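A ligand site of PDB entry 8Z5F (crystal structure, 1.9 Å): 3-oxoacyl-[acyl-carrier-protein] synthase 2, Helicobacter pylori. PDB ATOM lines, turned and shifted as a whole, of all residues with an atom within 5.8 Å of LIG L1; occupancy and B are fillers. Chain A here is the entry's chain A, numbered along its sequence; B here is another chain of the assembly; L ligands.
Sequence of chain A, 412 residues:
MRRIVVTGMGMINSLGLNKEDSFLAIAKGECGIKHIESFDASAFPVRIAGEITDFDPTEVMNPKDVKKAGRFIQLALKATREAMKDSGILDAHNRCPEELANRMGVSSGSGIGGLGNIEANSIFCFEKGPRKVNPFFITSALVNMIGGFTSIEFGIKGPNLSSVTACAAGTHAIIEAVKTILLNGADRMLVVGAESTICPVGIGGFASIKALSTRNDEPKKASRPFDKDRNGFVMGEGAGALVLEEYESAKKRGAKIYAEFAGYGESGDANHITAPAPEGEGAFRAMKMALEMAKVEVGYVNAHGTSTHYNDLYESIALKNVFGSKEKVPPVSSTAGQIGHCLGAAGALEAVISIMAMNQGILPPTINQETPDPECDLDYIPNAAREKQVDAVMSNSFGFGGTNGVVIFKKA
CA of Gly 111 touches C6 of LIG L1 (3.8 Å). Ile 112 touches LIG L1. Leu 115 touches LIG L1. Ala 166 touches LIG L1. Phe 206 touches LIG L1. Leu 343 touches LIG L1. Phe 398 touches LIG L1 (O to O1, 3.9 Å). Gly 399 touches LIG L1. Ile 138 of chain B touches LIG L1 (CG1 to C10, 3.9 Å). CD1 of Leu 142 of chain B touches C4 of LIG L1, 3.8 Å away. Within 4 Å of LIG L1: Gly 111, Ile 112, Leu 115, Ala 166, Cys 167, Phe 206, Leu 343, Phe 398, Gly 399, Phe 400, Ile 138 of chain B and Leu 142 of chain B.
O1 of LIG L1 lies within hydrogen-bond range of N of Cys 167 (2.6 Å). A carbon (C1) of LIG L1 is bonded to the side-chain sulfur of Cys 167 (1.8 Å). An oxygen (O1) of LIG L1 sits at hydrogen-bond distance from the backbone NH (N) of Phe 400.
SG of Cys 167 is in hydrogen-bond range of NE2 of His 341, at 3.3 Å. OE2 of Glu 195 is in hydrogen-bond range of N of Ile 112, at 3.1 Å. The side-chain carboxylate (OE1) of Glu 195 lies within hydrogen-bond range of the backbone NH (N) of Gly 111, at 2.9 Å. NE2 of His 304 sits at hydrogen-bond distance from O of Phe 398 (2.9 Å). NE2 of His 341 sits close to N of Leu 343, at 3.1 Å.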
ATOM      1  N   GLY A 111      -5.177  -2.726   6.464  1.00  0.00           N
ATOM      2  CA  GLY A 111      -4.818  -2.092   7.747  1.00  0.00           C
ATOM      3  C   GLY A 111      -5.837  -2.363   8.845  1.00  0.00           C
ATOM      4  O   GLY A 111      -5.399  -2.698   9.970  1.00  0.00           O
ATOM      5  N   ILE A 112      -7.138  -2.215   8.560  1.00  0.00           N
ATOM      6  CA  ILE A 112      -8.174  -2.371   9.618  1.00  0.00           C
ATOM      7  C   ILE A 112      -9.376  -3.149   9.072  1.00  0.00           C
ATOM      8  O   ILE A 112     -10.162  -3.661   9.885  1.00  0.00           O
ATOM      9  CB  ILE A 112      -8.603  -1.001  10.187  1.00  0.00           C
ATOM     10  CG1 ILE A 112      -9.281  -1.132  11.550  1.00  0.00           C
ATOM     11  CG2 ILE A 112      -9.477  -0.265   9.183  1.00  0.00           C
ATOM     12  CD1 ILE A 112      -9.586   0.190  12.201  1.00  0.00           C
ATOM     13  N   LEU A 115     -13.880  -1.287   8.980  1.00  0.00           N
ATOM     14  CA  LEU A 115     -14.038  -0.290  10.079  1.00  0.00           C
ATOM     15  C   LEU A 115     -15.496   0.183  10.144  1.00  0.00           C
ATOM     16  O   LEU A 115     -16.053   0.169  11.237  1.00  0.00           O
ATOM     17  CB  LEU A 115     -13.121   0.911   9.858  1.00  0.00           C
ATOM     18  CG  LEU A 115     -13.244   2.016  10.901  1.00  0.00           C
ATOM     19  CD1 LEU A 115     -12.985   1.462  12.294  1.00  0.00           C
ATOM     20  CD2 LEU A 115     -12.288   3.151  10.583  1.00  0.00           C
ATOM     21  N   THR A 165      -0.006  -4.969   8.527  1.00  0.00           N
ATOM     22  CA  THR A 165       0.992  -3.955   8.881  1.00  0.00           C
ATOM     23  C   THR A 165       0.658  -2.563   8.359  1.00  0.00           C
ATOM     24  O   THR A 165       1.476  -1.936   7.694  1.00  0.00           O
ATOM     25  CB  THR A 165       2.373  -4.365   8.374  1.00  0.00           C
ATOM     26  OG1 THR A 165       2.243  -5.109   7.154  1.00  0.00           O
ATOM     27  CG2 THR A 165       3.166  -5.165   9.464  1.00  0.00           C
ATOM     28  N   ALA A 166      -0.545  -2.065   8.701  1.00  0.00           N
ATOM     29  CA  ALA A 166      -0.863  -0.656   8.517  1.00  0.00           C
ATOM     30  C   ALA A 166      -0.685  -0.215   7.055  1.00  0.00           C
ATOM     31  O   ALA A 166      -1.141  -0.921   6.164  1.00  0.00           O
ATOM     32  CB  ALA A 166      -0.007   0.193   9.466  1.00  0.00           C
ATOM     33  N   CYS A 167      -0.045   0.913   6.795  1.00  0.00           N
ATOM     34  CA  CYS A 167       0.039   1.416   5.402  1.00  0.00           C
ATOM     35  C   CYS A 167       1.055   0.583   4.579  1.00  0.00           C
ATOM     36  O   CYS A 167       1.163   0.805   3.364  1.00  0.00           O
ATOM     37  CB  CYS A 167       0.256   2.921   5.407  1.00  0.00           C
ATOM     38  SG  CYS A 167      -0.958   3.886   6.309  1.00  0.00           S
ATOM     39  N   ALA A 168       1.756  -0.357   5.188  1.00  0.00           N
ATOM     40  CA  ALA A 168       2.636  -1.228   4.407  1.00  0.00           C
ATOM     41  C   ALA A 168       2.060  -2.644   4.206  1.00  0.00           C
ATOM     42  O   ALA A 168       2.738  -3.514   3.656  1.00  0.00           O
ATOM     43  CB  ALA A 168       4.019  -1.292   5.044  1.00  0.00           C
ATOM     44  N   GLU A 195      -8.579  -1.789   0.869  1.00  0.00           N
ATOM     45  CA  GLU A 195      -8.944  -0.937   1.990  1.00  0.00           C
ATOM     46  C   GLU A 195     -10.092  -0.038   1.597  1.00  0.00           C
ATOM     47  O   GLU A 195     -10.141   0.469   0.464  1.00  0.00           O
ATOM     48  CB  GLU A 195      -7.763  -0.095   2.483  1.00  0.00           C
ATOM     49  CG  GLU A 195      -7.978   0.522   3.871  1.00  0.00           C
ATOM     50  CD  GLU A 195      -7.289  -0.262   4.996  1.00  0.00           C
ATOM     51  OE1 GLU A 195      -6.046  -0.440   4.931  1.00  0.00           O
ATOM     52  OE2 GLU A 195      -8.002  -0.715   5.931  1.00  0.00           O
ATOM     53  N   THR A 197     -12.095   2.763   4.125  1.00  0.00           N
ATOM     54  CA  THR A 197     -12.323   3.276   5.473  1.00  0.00           C
ATOM     55  C   THR A 197     -12.812   4.719   5.457  1.00  0.00           C
ATOM     56  O   THR A 197     -12.569   5.469   6.412  1.00  0.00           O
ATOM     57  CB  THR A 197     -11.068   3.184   6.320  1.00  0.00           C
ATOM     58  OG1 THR A 197     -10.014   3.904   5.659  1.00  0.00           O
ATOM     59  CG2 THR A 197     -10.672   1.732   6.538  1.00  0.00           C
ATOM     60  N   VAL A 201     -15.692   7.500  11.745  1.00  0.00           N
ATOM     61  CA  VAL A 201     -14.618   7.279  12.728  1.00  0.00           C
ATOM     62  C   VAL A 201     -13.258   7.121  12.034  1.00  0.00           C
ATOM     63  O   VAL A 201     -12.218   7.420  12.630  1.00  0.00           O
ATOM     64  CB  VAL A 201     -14.940   6.073  13.628  1.00  0.00           C
ATOM     65  CG1 VAL A 201     -14.562   4.761  12.950  1.00  0.00           C
ATOM     66  CG2 VAL A 201     -14.225   6.205  14.986  1.00  0.00           C
ATOM     67  N   GLY A 202     -13.269   6.678  10.793  1.00  0.00           N
ATOM     68  CA  GLY A 202     -11.972   6.626  10.113  1.00  0.00           C
ATOM     69  C   GLY A 202     -11.446   7.999   9.782  1.00  0.00           C
ATOM     70  O   GLY A 202     -10.275   8.272  10.063  1.00  0.00           O
ATOM     71  N   PHE A 206      -8.012  10.033  11.765  1.00  0.00           N
ATOM     72  CA  PHE A 206      -6.816  10.605  11.123  1.00  0.00           C
ATOM     73  C   PHE A 206      -6.810  12.130  11.260  1.00  0.00           C
ATOM     74  O   PHE A 206      -5.743  12.738  11.276  1.00  0.00           O
ATOM     75  CB  PHE A 206      -6.733  10.167   9.664  1.00  0.00           C
ATOM     76  CG  PHE A 206      -6.166   8.792   9.445  1.00  0.00           C
ATOM     77  CD1 PHE A 206      -4.847   8.523   9.752  1.00  0.00           C
ATOM     78  CD2 PHE A 206      -6.946   7.776   8.924  1.00  0.00           C
ATOM     79  CE1 PHE A 206      -4.316   7.256   9.550  1.00  0.00           C
ATOM     80  CE2 PHE A 206      -6.422   6.520   8.717  1.00  0.00           C
ATOM     81  CZ  PHE A 206      -5.110   6.257   9.028  1.00  0.00           C
ATOM     82  N   PHE A 233      -2.194  13.799   4.182  1.00  0.00           N
ATOM     83  CA  PHE A 233      -2.583  12.940   3.079  1.00  0.00           C
ATOM     84  C   PHE A 233      -4.077  13.064   2.833  1.00  0.00           C
ATOM     85  O   PHE A 233      -4.814  13.683   3.593  1.00  0.00           O
ATOM     86  CB  PHE A 233      -2.145  11.478   3.315  1.00  0.00           C
ATOM     87  CG  PHE A 233      -2.948  10.717   4.342  1.00  0.00           C
ATOM     88  CD1 PHE A 233      -2.627  10.799   5.687  1.00  0.00           C
ATOM     89  CD2 PHE A 233      -3.943   9.838   3.940  1.00  0.00           C
ATOM     90  CE1 PHE A 233      -3.326  10.039   6.656  1.00  0.00           C
ATOM     91  CE2 PHE A 233      -4.647   9.067   4.888  1.00  0.00           C
ATOM     92  CZ  PHE A 233      -4.342   9.170   6.248  1.00  0.00           C
ATOM     93  N   MET A 235      -7.237  10.446   2.071  1.00  0.00           N
ATOM     94  CA  MET A 235      -7.497   9.017   2.220  1.00  0.00           C
ATOM     95  C   MET A 235      -8.164   8.504   0.966  1.00  0.00           C
ATOM     96  O   MET A 235      -9.154   9.071   0.506  1.00  0.00           O
ATOM     97  CB  MET A 235      -8.364   8.734   3.463  1.00  0.00           C
ATOM     98  CG  MET A 235      -9.076   7.353   3.445  1.00  0.00           C
ATOM     99  SD  MET A 235     -10.209   7.057   4.857  1.00  0.00           S
ATOM    100  CE  MET A 235      -9.236   7.590   6.261  1.00  0.00           C
ATOM    101  N   HIS A 304       6.264   5.763  -1.486  1.00  0.00           N
ATOM    102  CA  HIS A 304       5.049   5.769  -0.625  1.00  0.00           C
ATOM    103  C   HIS A 304       4.455   7.163  -0.818  1.00  0.00           C
ATOM    104  O   HIS A 304       3.281   7.257  -1.225  1.00  0.00           O
ATOM    105  CB  HIS A 304       5.396   5.370   0.811  1.00  0.00           C
ATOM    106  CG  HIS A 304       4.255   4.942   1.662  1.00  0.00           C
ATOM    107  ND1 HIS A 304       3.363   3.957   1.297  1.00  0.00           N
ATOM    108  CD2 HIS A 304       3.871   5.357   2.881  1.00  0.00           C
ATOM    109  CE1 HIS A 304       2.474   3.805   2.276  1.00  0.00           C
ATOM    110  NE2 HIS A 304       2.768   4.646   3.236  1.00  0.00           N
ATOM    111  N   HIS A 341      -3.877   8.388  -0.818  1.00  0.00           N
ATOM    112  CA  HIS A 341      -3.079   7.308  -0.160  1.00  0.00           C
ATOM    113  C   HIS A 341      -4.068   6.247   0.338  1.00  0.00           C
ATOM    114  O   HIS A 341      -4.841   6.560   1.243  1.00  0.00           O
ATOM    115  CB  HIS A 341      -2.205   7.829   0.970  1.00  0.00           C
ATOM    116  CG  HIS A 341      -1.722   6.688   1.795  1.00  0.00           C
ATOM    117  ND1 HIS A 341      -0.734   5.833   1.354  1.00  0.00           N
ATOM    118  CD2 HIS A 341      -2.099   6.225   2.984  1.00  0.00           C
ATOM    119  CE1 HIS A 341      -0.518   4.905   2.268  1.00  0.00           C
ATOM    120  NE2 HIS A 341      -1.336   5.128   3.266  1.00  0.00           N
ATOM    121  N   LEU A 343      -3.716   3.546   2.043  1.00  0.00           N
ATOM    122  CA  LEU A 343      -3.361   2.776   3.266  1.00  0.00           C
ATOM    123  C   LEU A 343      -3.037   1.309   2.945  1.00  0.00           C
ATOM    124  O   LEU A 343      -2.205   1.068   2.058  1.00  0.00           O
ATOM    125  CB  LEU A 343      -4.553   2.886   4.217  1.00  0.00           C
ATOM    126  CG  LEU A 343      -5.075   4.298   4.476  1.00  0.00           C
ATOM    127  CD1 LEU A 343      -6.449   4.259   5.124  1.00  0.00           C
ATOM    128  CD2 LEU A 343      -4.104   5.079   5.354  1.00  0.00           C
ATOM    129  N   GLY A 344      -3.659   0.374   3.674  1.00  0.00           N
ATOM    130  CA  GLY A 344      -3.369  -1.075   3.502  1.00  0.00           C
ATOM    131  C   GLY A 344      -3.280  -1.490   2.049  1.00  0.00           C
ATOM    132  O   GLY A 344      -2.409  -2.320   1.735  1.00  0.00           O
ATOM    133  N   PHE A 398       5.515   2.227   3.950  1.00  0.00           N
ATOM    134  CA  PHE A 398       5.792   2.356   5.378  1.00  0.00           C
ATOM    135  C   PHE A 398       4.490   2.534   6.138  1.00  0.00           C
ATOM    136  O   PHE A 398       3.522   3.121   5.644  1.00  0.00           O
ATOM    137  CB  PHE A 398       6.751   3.544   5.647  1.00  0.00           C
ATOM    138  CG  PHE A 398       7.766   3.768   4.552  1.00  0.00           C
ATOM    139  CD1 PHE A 398       8.675   2.779   4.221  1.00  0.00           C
ATOM    140  CD2 PHE A 398       7.789   4.976   3.843  1.00  0.00           C
ATOM    141  CE1 PHE A 398       9.608   2.969   3.197  1.00  0.00           C
ATOM    142  CE2 PHE A 398       8.715   5.177   2.815  1.00  0.00           C
ATOM    143  CZ  PHE A 398       9.617   4.176   2.487  1.00  0.00           C
ATOM    144  N   GLY A 399       4.466   2.037   7.377  1.00  0.00           N
ATOM    145  CA  GLY A 399       3.254   2.074   8.173  1.00  0.00           C
ATOM    146  C   GLY A 399       3.515   2.503   9.600  1.00  0.00           C
ATOM    147  O   GLY A 399       4.645   2.422  10.115  1.00  0.00           O
ATOM    148  N   PHE A 400       2.407   2.908  10.249  1.00  0.00           N
ATOM    149  CA  PHE A 400       2.438   3.220  11.693  1.00  0.00           C
ATOM    150  C   PHE A 400       3.116   2.045  12.401  1.00  0.00           C
ATOM    151  O   PHE A 400       2.949   0.900  11.954  1.00  0.00           O
ATOM    152  CB  PHE A 400       1.022   3.518  12.178  1.00  0.00           C
ATOM    153  CG  PHE A 400       0.487   4.894  11.887  1.00  0.00           C
ATOM    154  CD1 PHE A 400       1.281   5.865  11.302  1.00  0.00           C
ATOM    155  CD2 PHE A 400      -0.819   5.219  12.208  1.00  0.00           C
ATOM    156  CE1 PHE A 400       0.784   7.121  11.048  1.00  0.00           C
ATOM    157  CE2 PHE A 400      -1.315   6.481  11.946  1.00  0.00           C
ATOM    158  CZ  PHE A 400      -0.520   7.434  11.362  1.00  0.00           C
ATOM    159  N   PHE B 137      -6.518   6.991  19.406  1.00  0.00           N
ATOM    160  CA  PHE B 137      -7.404   5.887  18.952  1.00  0.00           C
ATOM    161  C   PHE B 137      -6.711   4.941  17.971  1.00  0.00           C
ATOM    162  O   PHE B 137      -6.573   3.773  18.304  1.00  0.00           O
ATOM    163  CB  PHE B 137      -8.663   6.444  18.300  1.00  0.00           C
ATOM    164  CG  PHE B 137      -9.411   5.485  17.410  1.00  0.00           C
ATOM    165  CD1 PHE B 137      -9.708   4.204  17.843  1.00  0.00           C
ATOM    166  CD2 PHE B 137      -9.834   5.858  16.152  1.00  0.00           C
ATOM    167  CE1 PHE B 137     -10.394   3.315  17.032  1.00  0.00           C
ATOM    168  CE2 PHE B 137     -10.528   4.981  15.337  1.00  0.00           C
ATOM    169  CZ  PHE B 137     -10.798   3.713  15.780  1.00  0.00           C
ATOM    170  N   ILE B 138      -6.275   5.447  16.817  1.00  0.00           N
ATOM    171  CA  ILE B 138      -5.762   4.520  15.758  1.00  0.00           C
ATOM    172  C   ILE B 138      -4.603   3.661  16.255  1.00  0.00           C
ATOM    173  O   ILE B 138      -4.676   2.427  16.132  1.00  0.00           O
ATOM    174  CB  ILE B 138      -5.388   5.292  14.474  1.00  0.00           C
ATOM    175  CG1 ILE B 138      -6.613   5.966  13.836  1.00  0.00           C
ATOM    176  CG2 ILE B 138      -4.662   4.393  13.493  1.00  0.00           C
ATOM    177  CD1 ILE B 138      -6.262   6.923  12.728  1.00  0.00           C
ATOM    178  N   LEU B 142      -4.694  -0.743  16.103  1.00  0.00           N
ATOM    179  CA  LEU B 142      -4.205  -1.495  14.961  1.00  0.00           C
ATOM    180  C   LEU B 142      -3.463  -2.736  15.435  1.00  0.00           C
ATOM    181  O   LEU B 142      -2.648  -2.664  16.352  1.00  0.00           O
ATOM    182  CB  LEU B 142      -3.270  -0.649  14.089  1.00  0.00           C
ATOM    183  CG  LEU B 142      -3.820   0.607  13.422  1.00  0.00           C
ATOM    184  CD1 LEU B 142      -2.723   1.350  12.653  1.00  0.00           C
ATOM    185  CD2 LEU B 142      -4.968   0.256  12.509  1.00  0.00           C
HETATM  186  C1  LIG L   1      -0.293   3.778   7.935  1.00  0.00           C
HETATM  187  O1  LIG L   1       0.599   3.029   8.232  1.00  0.00           O
HETATM  188  C2  LIG L   1      -0.950   4.716   8.922  1.00  0.00           C
HETATM  189  C3  LIG L   1      -2.427   4.499   8.984  1.00  0.00           C
HETATM  190  C4  LIG L   1      -2.795   3.083   9.326  1.00  0.00           C
HETATM  191  C5  LIG L   1      -3.629   2.430   8.225  1.00  0.00           C
HETATM  192  C6  LIG L   1      -4.790   1.619   8.765  1.00  0.00           C
HETATM  193  C7  LIG L   1      -6.141   2.254   8.518  1.00  0.00           C
HETATM  194  C8  LIG L   1      -7.000   2.359   9.764  1.00  0.00           C
HETATM  195  C9  LIG L   1      -7.927   3.556   9.812  1.00  0.00           C
HETATM  196  C10 LIG L   1      -8.500   3.835  11.186  1.00  0.00           C
HETATM  197  O1  LG2 L   2       4.181  11.982  13.003  1.00  0.00           O
HETATM  198  O2  LG2 L   2       3.370  12.152  10.245  1.00  0.00           O
HETATM  199  C1  LG2 L   2       1.820  12.552  12.922  1.00  0.00           C
HETATM  200  C2  LG2 L   2       2.073  12.992  14.344  1.00  0.00           C
HETATM  201  P1  LG2 L   2       4.042  14.242  15.405  1.00  0.00           P
HETATM  202  O3  LG2 L   2       4.959  15.365  15.051  1.00  0.00           O
HETATM  203  O4  LG2 L   2       4.565  12.842  15.404  1.00  0.00           O
HETATM  204  O5  LG2 L   2       2.813  14.201  14.396  1.00  0.00           O
HETATM  205  C3  LG2 L   2       0.495  11.814  12.850  1.00  0.00           C
HETATM  206  C4  LG2 L   2       1.765  13.765  12.015  1.00  0.00           C
HETATM  207  C5  LG2 L   2       2.905  11.539  12.529  1.00  0.00           C
HETATM  208  C6  LG2 L   2       2.950  11.331  11.041  1.00  0.00           C
HETATM  209  N1  LG2 L   2       2.511  10.158  10.639  1.00  0.00           N
HETATM  210  C7  LG2 L   2       2.431   9.726   9.266  1.00  0.00           C
HETATM  211  C8  LG2 L   2       3.804   9.269   8.811  1.00  0.00           C
HETATM  212  C9  LG2 L   2       3.452   8.693   7.485  1.00  0.00           C
HETATM  213  O6  LG2 L   2       3.545   9.379   6.502  1.00  0.00           O
HETATM  214  N2  LG2 L   2       2.967   7.464   7.450  1.00  0.00           N
HETATM  215  C10 LG2 L   2       2.548   6.761   6.251  1.00  0.00           C
HETATM  216  C11 LG2 L   2       1.063   6.512   6.451  1.00  0.00           C
HETATM  217  S1  LG2 L   2       0.085   8.026   6.647  1.00  0.00           S
